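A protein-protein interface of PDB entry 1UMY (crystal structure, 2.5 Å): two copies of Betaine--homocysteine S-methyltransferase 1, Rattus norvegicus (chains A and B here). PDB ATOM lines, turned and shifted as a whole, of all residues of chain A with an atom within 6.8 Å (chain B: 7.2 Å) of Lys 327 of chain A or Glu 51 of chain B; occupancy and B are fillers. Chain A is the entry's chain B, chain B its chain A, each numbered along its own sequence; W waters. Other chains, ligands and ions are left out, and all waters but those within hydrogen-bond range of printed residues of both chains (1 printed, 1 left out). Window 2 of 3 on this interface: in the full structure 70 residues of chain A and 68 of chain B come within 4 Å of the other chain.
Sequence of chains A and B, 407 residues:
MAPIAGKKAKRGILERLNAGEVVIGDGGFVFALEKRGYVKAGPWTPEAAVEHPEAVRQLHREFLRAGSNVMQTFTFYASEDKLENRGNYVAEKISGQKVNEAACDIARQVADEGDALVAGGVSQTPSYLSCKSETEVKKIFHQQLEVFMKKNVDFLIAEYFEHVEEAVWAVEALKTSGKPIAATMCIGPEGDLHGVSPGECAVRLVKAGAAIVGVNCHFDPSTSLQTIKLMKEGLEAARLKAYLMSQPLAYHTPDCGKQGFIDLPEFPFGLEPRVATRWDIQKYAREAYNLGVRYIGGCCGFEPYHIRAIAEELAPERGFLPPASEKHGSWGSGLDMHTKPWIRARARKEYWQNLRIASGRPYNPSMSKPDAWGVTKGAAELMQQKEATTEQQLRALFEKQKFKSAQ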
ATOM      1  N   ARG A  65       7.342  -7.838 -33.138  1.00  0.00           N
ATOM      2  CA  ARG A  65       5.926  -7.528 -33.236  1.00  0.00           C
ATOM      3  C   ARG A  65       5.664  -6.124 -32.735  1.00  0.00           C
ATOM      4  O   ARG A  65       4.773  -5.433 -33.228  1.00  0.00           O
ATOM      5  CB  ARG A  65       5.117  -8.531 -32.416  1.00  0.00           C
ATOM      6  CG  ARG A  65       3.621  -8.308 -32.435  1.00  0.00           C
ATOM      7  CD  ARG A  65       2.920  -9.491 -31.772  1.00  0.00           C
ATOM      8  NE  ARG A  65       1.474  -9.314 -31.604  1.00  0.00           N
ATOM      9  CZ  ARG A  65       0.583  -9.297 -32.593  1.00  0.00           C
ATOM     10  NH1 ARG A  65      -0.701  -9.132 -32.316  1.00  0.00           N
ATOM     11  NH2 ARG A  65       0.964  -9.445 -33.851  1.00  0.00           N
ATOM     12  N   ARG A 278       4.102   3.228 -20.568  1.00  0.00           N
ATOM     13  CA  ARG A 278       4.110   3.419 -22.011  1.00  0.00           C
ATOM     14  C   ARG A 278       4.104   4.904 -22.329  1.00  0.00           C
ATOM     15  O   ARG A 278       4.785   5.352 -23.241  1.00  0.00           O
ATOM     16  CB  ARG A 278       2.907   2.721 -22.656  1.00  0.00           C
ATOM     17  CG  ARG A 278       1.540   3.225 -22.234  1.00  0.00           C
ATOM     18  CD  ARG A 278       0.488   2.163 -22.524  1.00  0.00           C
ATOM     19  NE  ARG A 278       0.730   0.968 -21.719  1.00  0.00           N
ATOM     20  CZ  ARG A 278       0.297  -0.252 -22.019  1.00  0.00           C
ATOM     21  NH1 ARG A 278      -0.409  -0.460 -23.119  1.00  0.00           N
ATOM     22  NH2 ARG A 278       0.578  -1.265 -21.214  1.00  0.00           N
ATOM     23  N   ARG A 308       6.755  -0.756 -28.316  1.00  0.00           N
ATOM     24  CA  ARG A 308       5.532  -0.416 -29.009  1.00  0.00           C
ATOM     25  C   ARG A 308       5.132   1.035 -28.778  1.00  0.00           C
ATOM     26  O   ARG A 308       4.430   1.623 -29.594  1.00  0.00           O
ATOM     27  CB  ARG A 308       4.401  -1.323 -28.561  1.00  0.00           C
ATOM     28  CG  ARG A 308       3.074  -0.978 -29.211  1.00  0.00           C
ATOM     29  CD  ARG A 308       1.970  -1.085 -28.206  1.00  0.00           C
ATOM     30  NE  ARG A 308       1.364  -2.399 -28.192  1.00  0.00           N
ATOM     31  CZ  ARG A 308       0.651  -2.871 -27.183  1.00  0.00           C
ATOM     32  NH1 ARG A 308       0.474  -2.136 -26.105  1.00  0.00           N
ATOM     33  NH2 ARG A 308       0.094  -4.070 -27.270  1.00  0.00           N
ATOM     34  N   GLU A 312       4.514   3.733 -31.798  1.00  0.00           N
ATOM     35  CA  GLU A 312       3.209   4.356 -31.923  1.00  0.00           C
ATOM     36  C   GLU A 312       3.330   5.878 -31.899  1.00  0.00           C
ATOM     37  O   GLU A 312       2.638   6.575 -32.637  1.00  0.00           O
ATOM     38  CB  GLU A 312       2.275   3.879 -30.805  1.00  0.00           C
ATOM     39  CG  GLU A 312       1.954   2.387 -30.866  1.00  0.00           C
ATOM     40  CD  GLU A 312       0.861   1.961 -29.905  1.00  0.00           C
ATOM     41  OE1 GLU A 312       0.565   2.714 -28.962  1.00  0.00           O
ATOM     42  OE2 GLU A 312       0.310   0.865 -30.092  1.00  0.00           O
ATOM     43  N   PRO A 323       2.779  -4.264 -35.924  1.00  0.00           N
ATOM     44  CA  PRO A 323       1.697  -5.220 -35.719  1.00  0.00           C
ATOM     45  C   PRO A 323       1.112  -5.227 -34.310  1.00  0.00           C
ATOM     46  O   PRO A 323      -0.101  -5.181 -34.148  1.00  0.00           O
ATOM     47  CB  PRO A 323       2.326  -6.556 -36.125  1.00  0.00           C
ATOM     48  CG  PRO A 323       3.786  -6.297 -36.152  1.00  0.00           C
ATOM     49  CD  PRO A 323       3.912  -4.897 -36.607  1.00  0.00           C
ATOM     50  N   ALA A 324       1.963  -5.259 -33.291  1.00  0.00           N
ATOM     51  CA  ALA A 324       1.493  -5.282 -31.911  1.00  0.00           C
ATOM     52  C   ALA A 324       0.362  -4.292 -31.606  1.00  0.00           C
ATOM     53  O   ALA A 324      -0.436  -4.529 -30.699  1.00  0.00           O
ATOM     54  CB  ALA A 324       2.649  -5.043 -30.967  1.00  0.00           C
ATOM     55  N   SER A 325       0.289  -3.189 -32.352  1.00  0.00           N
ATOM     56  CA  SER A 325      -0.759  -2.201 -32.127  1.00  0.00           C
ATOM     57  C   SER A 325      -2.153  -2.778 -32.369  1.00  0.00           C
ATOM     58  O   SER A 325      -3.159  -2.156 -32.031  1.00  0.00           O
ATOM     59  CB  SER A 325      -0.536  -0.986 -33.011  1.00  0.00           C
ATOM     60  OG  SER A 325       0.513  -0.191 -32.493  1.00  0.00           O
ATOM     61  N   GLU A 326      -2.202  -3.973 -32.952  1.00  0.00           N
ATOM     62  CA  GLU A 326      -3.464  -4.641 -33.231  1.00  0.00           C
ATOM     63  C   GLU A 326      -4.199  -4.889 -31.931  1.00  0.00           C
ATOM     64  O   GLU A 326      -5.427  -4.870 -31.886  1.00  0.00           O
ATOM     65  CB  GLU A 326      -3.223  -5.987 -33.905  1.00  0.00           C
ATOM     66  CG  GLU A 326      -2.899  -5.932 -35.388  1.00  0.00           C
ATOM     67  CD  GLU A 326      -2.442  -7.287 -35.920  1.00  0.00           C
ATOM     68  OE1 GLU A 326      -3.087  -8.310 -35.568  1.00  0.00           O
ATOM     69  OE2 GLU A 326      -1.442  -7.319 -36.684  1.00  0.00           O
ATOM     70  N   LYS A 327      -3.442  -5.139 -30.869  1.00  0.00           N
ATOM     71  CA  LYS A 327      -4.042  -5.418 -29.576  1.00  0.00           C
ATOM     72  C   LYS A 327      -3.876  -4.225 -28.665  1.00  0.00           C
ATOM     73  O   LYS A 327      -3.684  -4.367 -27.469  1.00  0.00           O
ATOM     74  CB  LYS A 327      -3.385  -6.648 -28.958  1.00  0.00           C
ATOM     75  CG  LYS A 327      -3.413  -7.890 -29.841  1.00  0.00           C
ATOM     76  CD  LYS A 327      -4.836  -8.334 -30.139  1.00  0.00           C
ATOM     77  CE  LYS A 327      -4.869  -9.586 -31.019  1.00  0.00           C
ATOM     78  NZ  LYS A 327      -6.263 -10.019 -31.356  1.00  0.00           N
ATOM     79  N   HIS A 328      -3.960  -3.039 -29.244  1.00  0.00           N
ATOM     80  CA  HIS A 328      -3.804  -1.811 -28.484  1.00  0.00           C
ATOM     81  C   HIS A 328      -4.771  -0.719 -28.965  1.00  0.00           C
ATOM     82  O   HIS A 328      -5.718  -0.985 -29.702  1.00  0.00           O
ATOM     83  CB  HIS A 328      -2.352  -1.315 -28.605  1.00  0.00           C
ATOM     84  CG  HIS A 328      -1.939  -0.370 -27.517  1.00  0.00           C
ATOM     85  ND1 HIS A 328      -1.034   0.647 -27.718  1.00  0.00           N
ATOM     86  CD2 HIS A 328      -2.311  -0.290 -26.218  1.00  0.00           C
ATOM     87  CE1 HIS A 328      -0.869   1.317 -26.593  1.00  0.00           C
ATOM     88  NE2 HIS A 328      -1.631   0.770 -25.668  1.00  0.00           N
ATOM     89  N   GLY A 329      -4.517   0.511 -28.533  1.00  0.00           N
ATOM     90  CA  GLY A 329      -5.344   1.640 -28.908  1.00  0.00           C
ATOM     91  C   GLY A 329      -4.494   2.885 -28.808  1.00  0.00           C
ATOM     92  O   GLY A 329      -3.373   2.811 -28.312  1.00  0.00           O
ATOM     93  N   LEU B  33       0.220 -10.966 -21.208  1.00  0.00           N
ATOM     94  CA  LEU B  33       0.097 -11.002 -22.654  1.00  0.00           C
ATOM     95  C   LEU B  33      -0.168  -9.620 -23.199  1.00  0.00           C
ATOM     96  O   LEU B  33       0.189  -9.319 -24.323  1.00  0.00           O
ATOM     97  CB  LEU B  33      -1.023 -11.948 -23.074  1.00  0.00           C
ATOM     98  CG  LEU B  33      -0.748 -13.444 -22.886  1.00  0.00           C
ATOM     99  CD1 LEU B  33      -1.908 -14.250 -23.447  1.00  0.00           C
ATOM    100  CD2 LEU B  33       0.533 -13.833 -23.616  1.00  0.00           C
ATOM    101  N   GLU B  34      -0.799  -8.769 -22.405  1.00  0.00           N
ATOM    102  CA  GLU B  34      -1.073  -7.420 -22.865  1.00  0.00           C
ATOM    103  C   GLU B  34       0.241  -6.678 -23.025  1.00  0.00           C
ATOM    104  O   GLU B  34       0.435  -5.958 -23.997  1.00  0.00           O
ATOM    105  CB  GLU B  34      -1.975  -6.677 -21.875  1.00  0.00           C
ATOM    106  CG  GLU B  34      -2.487  -5.334 -22.379  1.00  0.00           C
ATOM    107  CD  GLU B  34      -1.415  -4.264 -22.404  1.00  0.00           C
ATOM    108  OE1 GLU B  34      -1.526  -3.326 -23.222  1.00  0.00           O
ATOM    109  OE2 GLU B  34      -0.463  -4.344 -21.601  1.00  0.00           O
ATOM    110  N   GLY B  37       2.005  -7.837 -26.088  1.00  0.00           N
ATOM    111  CA  GLY B  37       1.368  -7.529 -27.357  1.00  0.00           C
ATOM    112  C   GLY B  37       0.402  -8.518 -27.991  1.00  0.00           C
ATOM    113  O   GLY B  37       0.251  -8.526 -29.205  1.00  0.00           O
ATOM    114  N   TYR B  38      -0.267  -9.332 -27.184  1.00  0.00           N
ATOM    115  CA  TYR B  38      -1.204 -10.314 -27.702  1.00  0.00           C
ATOM    116  C   TYR B  38      -2.623 -10.198 -27.146  1.00  0.00           C
ATOM    117  O   TYR B  38      -3.518 -10.903 -27.591  1.00  0.00           O
ATOM    118  CB  TYR B  38      -0.656 -11.716 -27.439  1.00  0.00           C
ATOM    119  CG  TYR B  38       0.703 -11.937 -28.061  1.00  0.00           C
ATOM    120  CD1 TYR B  38       0.840 -12.123 -29.436  1.00  0.00           C
ATOM    121  CD2 TYR B  38       1.858 -11.899 -27.282  1.00  0.00           C
ATOM    122  CE1 TYR B  38       2.087 -12.259 -30.007  1.00  0.00           C
ATOM    123  CE2 TYR B  38       3.105 -12.036 -27.845  1.00  0.00           C
ATOM    124  CZ  TYR B  38       3.215 -12.214 -29.204  1.00  0.00           C
ATOM    125  OH  TYR B  38       4.453 -12.348 -29.770  1.00  0.00           O
ATOM    126  N   VAL B  39      -2.832  -9.312 -26.182  1.00  0.00           N
ATOM    127  CA  VAL B  39      -4.149  -9.127 -25.594  1.00  0.00           C
ATOM    128  C   VAL B  39      -4.426  -7.643 -25.554  1.00  0.00           C
ATOM    129  O   VAL B  39      -3.630  -6.895 -25.020  1.00  0.00           O
ATOM    130  CB  VAL B  39      -4.209  -9.675 -24.163  1.00  0.00           C
ATOM    131  CG1 VAL B  39      -5.561  -9.421 -23.567  1.00  0.00           C
ATOM    132  CG2 VAL B  39      -3.914 -11.154 -24.164  1.00  0.00           C
ATOM    133  N   LYS B  40      -5.545  -7.214 -26.131  1.00  0.00           N
ATOM    134  CA  LYS B  40      -5.895  -5.799 -26.152  1.00  0.00           C
ATOM    135  C   LYS B  40      -6.578  -5.416 -24.866  1.00  0.00           C
ATOM    136  O   LYS B  40      -7.482  -6.101 -24.423  1.00  0.00           O
ATOM    137  CB  LYS B  40      -6.841  -5.506 -27.307  1.00  0.00           C
ATOM    138  CG  LYS B  40      -7.105  -4.028 -27.577  1.00  0.00           C
ATOM    139  CD  LYS B  40      -8.139  -3.883 -28.701  1.00  0.00           C
ATOM    140  CE  LYS B  40      -8.031  -2.569 -29.486  1.00  0.00           C
ATOM    141  NZ  LYS B  40      -8.358  -1.328 -28.714  1.00  0.00           N
ATOM    142  N   ALA B  41      -6.133  -4.332 -24.251  1.00  0.00           N
ATOM    143  CA  ALA B  41      -6.755  -3.870 -23.020  1.00  0.00           C
ATOM    144  C   ALA B  41      -8.068  -3.228 -23.452  1.00  0.00           C
ATOM    145  O   ALA B  41      -8.104  -2.467 -24.412  1.00  0.00           O
ATOM    146  CB  ALA B  41      -5.865  -2.853 -22.318  1.00  0.00           C
ATOM    147  N   THR B  45      -9.767 -10.041 -24.367  1.00  0.00           N
ATOM    148  CA  THR B  45     -10.096 -11.354 -24.866  1.00  0.00           C
ATOM    149  C   THR B  45      -8.911 -12.227 -25.211  1.00  0.00           C
ATOM    150  O   THR B  45      -7.837 -11.730 -25.490  1.00  0.00           O
ATOM    151  CB  THR B  45     -11.020 -11.223 -26.065  1.00  0.00           C
ATOM    152  OG1 THR B  45     -10.492 -10.245 -26.971  1.00  0.00           O
ATOM    153  CG2 THR B  45     -12.405 -10.792 -25.600  1.00  0.00           C
ATOM    154  N   PRO B  46      -9.103 -13.556 -25.204  1.00  0.00           N
ATOM    155  CA  PRO B  46      -8.069 -14.556 -25.505  1.00  0.00           C
ATOM    156  C   PRO B  46      -7.928 -15.098 -26.938  1.00  0.00           C
ATOM    157  O   PRO B  46      -7.396 -16.187 -27.131  1.00  0.00           O
ATOM    158  CB  PRO B  46      -8.412 -15.668 -24.529  1.00  0.00           C
ATOM    159  CG  PRO B  46      -9.906 -15.681 -24.611  1.00  0.00           C
ATOM    160  CD  PRO B  46     -10.278 -14.209 -24.587  1.00  0.00           C
ATOM    161  N   GLU B  47      -8.368 -14.354 -27.944  1.00  0.00           N
ATOM    162  CA  GLU B  47      -8.275 -14.854 -29.319  1.00  0.00           C
ATOM    163  C   GLU B  47      -6.860 -15.175 -29.801  1.00  0.00           C
ATOM    164  O   GLU B  47      -6.676 -15.644 -30.919  1.00  0.00           O
ATOM    165  CB  GLU B  47      -8.924 -13.874 -30.297  1.00  0.00           C
ATOM    166  CG  GLU B  47      -8.224 -12.547 -30.407  1.00  0.00           C
ATOM    167  CD  GLU B  47      -8.588 -11.603 -29.287  1.00  0.00           C
ATOM    168  OE1 GLU B  47      -8.196 -10.423 -29.375  1.00  0.00           O
ATOM    169  OE2 GLU B  47      -9.265 -12.036 -28.327  1.00  0.00           O
ATOM    170  N   ALA B  48      -5.863 -14.922 -28.968  1.00  0.00           N
ATOM    171  CA  ALA B  48      -4.490 -15.209 -29.349  1.00  0.00           C
ATOM    172  C   ALA B  48      -4.198 -16.706 -29.257  1.00  0.00           C
ATOM    173  O   ALA B  48      -3.221 -17.194 -29.819  1.00  0.00           O
ATOM    174  CB  ALA B  48      -3.537 -14.442 -28.463  1.00  0.00           C
ATOM    175  N   ALA B  49      -5.042 -17.433 -28.533  1.00  0.00           N
ATOM    176  CA  ALA B  49      -4.862 -18.873 -28.387  1.00  0.00           C
ATOM    177  C   ALA B  49      -4.899 -19.537 -29.761  1.00  0.00           C
ATOM    178  O   ALA B  49      -4.396 -20.637 -29.932  1.00  0.00           O
ATOM    179  CB  ALA B  49      -5.941 -19.453 -27.489  1.00  0.00           C
ATOM    180  N   VAL B  50      -5.498 -18.860 -30.736  1.00  0.00           N
ATOM    181  CA  VAL B  50      -5.560 -19.381 -32.093  1.00  0.00           C
ATOM    182  C   VAL B  50      -4.771 -18.495 -33.053  1.00  0.00           C
ATOM    183  O   VAL B  50      -4.270 -18.979 -34.067  1.00  0.00           O
ATOM    184  CB  VAL B  50      -7.022 -19.505 -32.622  1.00  0.00           C
ATOM    185  CG1 VAL B  50      -7.860 -20.275 -31.631  1.00  0.00           C
ATOM    186  CG2 VAL B  50      -7.622 -18.139 -32.895  1.00  0.00           C
ATOM    187  N   GLU B  51      -4.659 -17.206 -32.737  1.00  0.00           N
ATOM    188  CA  GLU B  51      -3.926 -16.265 -33.585  1.00  0.00           C
ATOM    189  C   GLU B  51      -2.419 -16.319 -33.349  1.00  0.00           C
ATOM    190  O   GLU B  51      -1.636 -16.067 -34.260  1.00  0.00           O
ATOM    191  CB  GLU B  51      -4.392 -14.831 -33.341  1.00  0.00           C
ATOM    192  CG  GLU B  51      -5.849 -14.577 -33.578  1.00  0.00           C
ATOM    193  CD  GLU B  51      -6.193 -13.113 -33.448  1.00  0.00           C
ATOM    194  OE1 GLU B  51      -5.549 -12.427 -32.626  1.00  0.00           O
ATOM    195  OE2 GLU B  51      -7.116 -12.639 -34.156  1.00  0.00           O
ATOM    196  N   HIS B  52      -2.013 -16.644 -32.126  1.00  0.00           N
ATOM    197  CA  HIS B  52      -0.601 -16.707 -31.776  1.00  0.00           C
ATOM    198  C   HIS B  52      -0.426 -17.738 -30.671  1.00  0.00           C
ATOM    199  O   HIS B  52      -0.055 -17.407 -29.550  1.00  0.00           O
ATOM    200  CB  HIS B  52      -0.137 -15.345 -31.257  1.00  0.00           C
ATOM    201  CG  HIS B  52      -0.615 -14.188 -32.078  1.00  0.00           C
ATOM    202  ND1 HIS B  52       0.052 -13.747 -33.202  1.00  0.00           N
ATOM    203  CD2 HIS B  52      -1.712 -13.403 -31.959  1.00  0.00           C
ATOM    204  CE1 HIS B  52      -0.614 -12.742 -33.739  1.00  0.00           C
ATOM    205  NE2 HIS B  52      -1.689 -12.513 -33.003  1.00  0.00           N
ATOM    206  N   PRO B  53      -0.693 -19.009 -30.973  1.00  0.00           N
ATOM    207  CA  PRO B  53      -0.553 -20.062 -29.965  1.00  0.00           C
ATOM    208  C   PRO B  53       0.827 -20.136 -29.306  1.00  0.00           C
ATOM    209  O   PRO B  53       0.942 -20.344 -28.100  1.00  0.00           O
ATOM    210  CB  PRO B  53      -0.904 -21.332 -30.749  1.00  0.00           C
ATOM    211  CG  PRO B  53      -0.490 -20.988 -32.146  1.00  0.00           C
ATOM    212  CD  PRO B  53      -1.014 -19.585 -32.289  1.00  0.00           C
ATOM    213  N   GLU B  54       1.875 -19.963 -30.102  1.00  0.00           N
ATOM    214  CA  GLU B  54       3.229 -20.047 -29.582  1.00  0.00           C
ATOM    215  C   GLU B  54       3.446 -19.068 -28.434  1.00  0.00           C
ATOM    216  O   GLU B  54       4.201 -19.346 -27.512  1.00  0.00           O
ATOM    217  CB  GLU B  54       4.252 -19.834 -30.718  1.00  0.00           C
ATOM    218  CG  GLU B  54       4.401 -18.410 -31.287  1.00  0.00           C
ATOM    219  CD  GLU B  54       3.121 -17.820 -31.884  1.00  0.00           C
ATOM    220  OE1 GLU B  54       2.365 -18.539 -32.585  1.00  0.00           O
ATOM    221  OE2 GLU B  54       2.893 -16.607 -31.658  1.00  0.00           O
ATOM    222  N   VAL B  56       0.947 -17.867 -26.281  1.00  0.00           N
ATOM    223  CA  VAL B  56       0.223 -18.403 -25.138  1.00  0.00           C
ATOM    224  C   VAL B  56       1.011 -19.575 -24.542  1.00  0.00           C
ATOM    225  O   VAL B  56       1.153 -19.698 -23.321  1.00  0.00           O
ATOM    226  CB  VAL B  56      -1.183 -18.885 -25.556  1.00  0.00           C
ATOM    227  CG1 VAL B  56      -1.984 -19.297 -24.338  1.00  0.00           C
ATOM    228  CG2 VAL B  56      -1.893 -17.787 -26.303  1.00  0.00           C
ATOM    229  N   VAL B  99     -11.662 -20.758 -29.964  1.00  0.00           N
ATOM    230  CA  VAL B  99     -10.664 -20.084 -29.167  1.00  0.00           C
ATOM    231  C   VAL B  99     -10.543 -20.848 -27.864  1.00  0.00           C
ATOM    232  O   VAL B  99      -9.497 -21.418 -27.549  1.00  0.00           O
ATOM    233  CB  VAL B  99     -11.098 -18.644 -28.874  1.00  0.00           C
ATOM    234  CG1 VAL B  99      -9.945 -17.856 -28.275  1.00  0.00           C
ATOM    235  CG2 VAL B  99     -11.590 -17.992 -30.149  1.00  0.00           C
ATOM    236  N   ALA B 102      -9.003 -24.220 -28.265  1.00  0.00           N
ATOM    237  CA  ALA B 102      -7.584 -24.143 -28.590  1.00  0.00           C
ATOM    238  C   ALA B 102      -6.809 -23.814 -27.322  1.00  0.00           C
ATOM    239  O   ALA B 102      -5.714 -24.317 -27.102  1.00  0.00           O
ATOM    240  CB  ALA B 102      -7.332 -23.080 -29.643  1.00  0.00           C
HETATM  241  O   HOH W   1      -3.806  -3.090 -25.076  1.00  0.00           O
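OE1 of Glu 34 of chain B lies within salt-bridge range of NH1 of Arg 278 of chain A, 3.1 Å away. The side-chain carboxylate of Glu 51 of chain B lies within salt-bridge range of the side-chain amino group of Lys 327 of chain A. OE1 of Glu 34 of chain B lies within salt-bridge range of NH1 of Arg 308 of chain A (3.7 Å). O of Gly 37 of chain B lies within hydrogen-bond range of NE of Arg 65 of chain A, at 2.8 Å. OE1 of Glu 47 of chain B lies within salt-bridge range of NZ of Lys 327 of chain A (2.8 Å). The backbone carbonyl oxygen (O) of His 328 of chain A lies close to the side-chain amino group (NZ) of Lys 40 of chain B.
The backbone carbonyl oxygen of Arg 65 of chain A is in hydrogen-bond range of the backbone NH of Ala 324 of chain A, at 2.8 Å. The guanidinium group of Arg 278 of chain A is in hydrogen-bond range of a ring nitrogen (NE2) of His 328 of chain A. The guanidinium group of Arg 308 of chain A lies within salt-bridge range of the side-chain carboxylate of Glu 312 of chain A (3.9 Å). The side-chain carboxylate (OE2) of Glu 47 of chain B lies within hydrogen-bond range of the side-chain hydroxyl (OG1) of Thr 45 of chain B (2.6 Å). O of Leu 33 of chain B lies within hydrogen-bond range of N of Tyr 38 of chain B (2.9 Å). OE2 of Glu 312 of chain A sits at hydrogen-bond distance from ND1 of His 328 of chain A, 2.7 Å away.
Tyr 38 of chain B touches Arg 65 of chain A (CE1 to CD, 3.4 Å). Arg 65 of chain A touches His 52 of chain B (NH1 to NE2, 3.6 Å). CA of Gly 37 of chain B touches NH2 of Arg 308 of chain A, 3.7 Å away. O of Gly 37 of chain B touches CG of Lys 327 of chain A, 3.8 Å away. Lys 327 of chain A touches Tyr 38 of chain B. Lys 327 of chain A touches Val 39 of chain B. Lys 40 of chain B touches Lys 327 of chain A (CA to O, 2.9 Å).
Of chain B, only Gly 37 (3.8 Å), Tyr 38 (3.6 Å), Val 39 (3.5 Å), Lys 40 (2.9 Å), Glu 47 (2.8 Å) and Glu 51 (2.8 Å) come within 4 Å of Lys 327 of chain A. Of chain A, only Lys 327 comes within 4 Å of Glu 51 of chain B. Of the printed residues of chain A, His 52 of chain B touches Arg 65. Printed residues of chain A within 4 Å of Lys 40 of chain B: Lys 327 (2.9 Å) and His 328 (2.8 Å). Printed residues of chain A within 4 Å of Glu 34 of chain B: Arg 278 (3.1 Å) and Arg 308 (3.7 Å). Ala 102 of chain B touches none of the printed residues of chain A. Val 99 of chain B touches none of the printed residues of chain A. The nearest residue of chain B that does not touch Lys 327 of chain A is Ala 41 of chain B (4.04 Å). The nearest printed residue of chain A that does not touch His 52 of chain B is Lys 327 of chain A (4.8 Å).
Of the 11 printed residues of chain A, 5 touch a printed residue of chain B. Of the 20 printed residues of chain B, 8 touch a printed residue of chain A. Hydrophobic or aromatic side chains of chain B within 4 Å of the printed part of chain A: Tyr 38 and His 52. Among the printed residues, 13 pairs touch across the chains. Among the printed residues, Asp or Glu carboxylates within 4 Å of a Lys or Arg side-chain nitrogen of the other chain: Arg 278 of chain A with Glu 34 of chain B, Arg 308 of chain A with Glu 34 of chain B, Lys 327 of chain A with Glu 47 of chain B and Lys 327 of chain A with Glu 51 of chain B.
No position is printed for both chains.
Water W1 lies within hydrogen-bond range of O of Lys 327 of chain A (2.7 Å), N of Ala 41 of chain B (2.8 Å) and OE1 of Glu 34 of chain B (2.9 Å).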
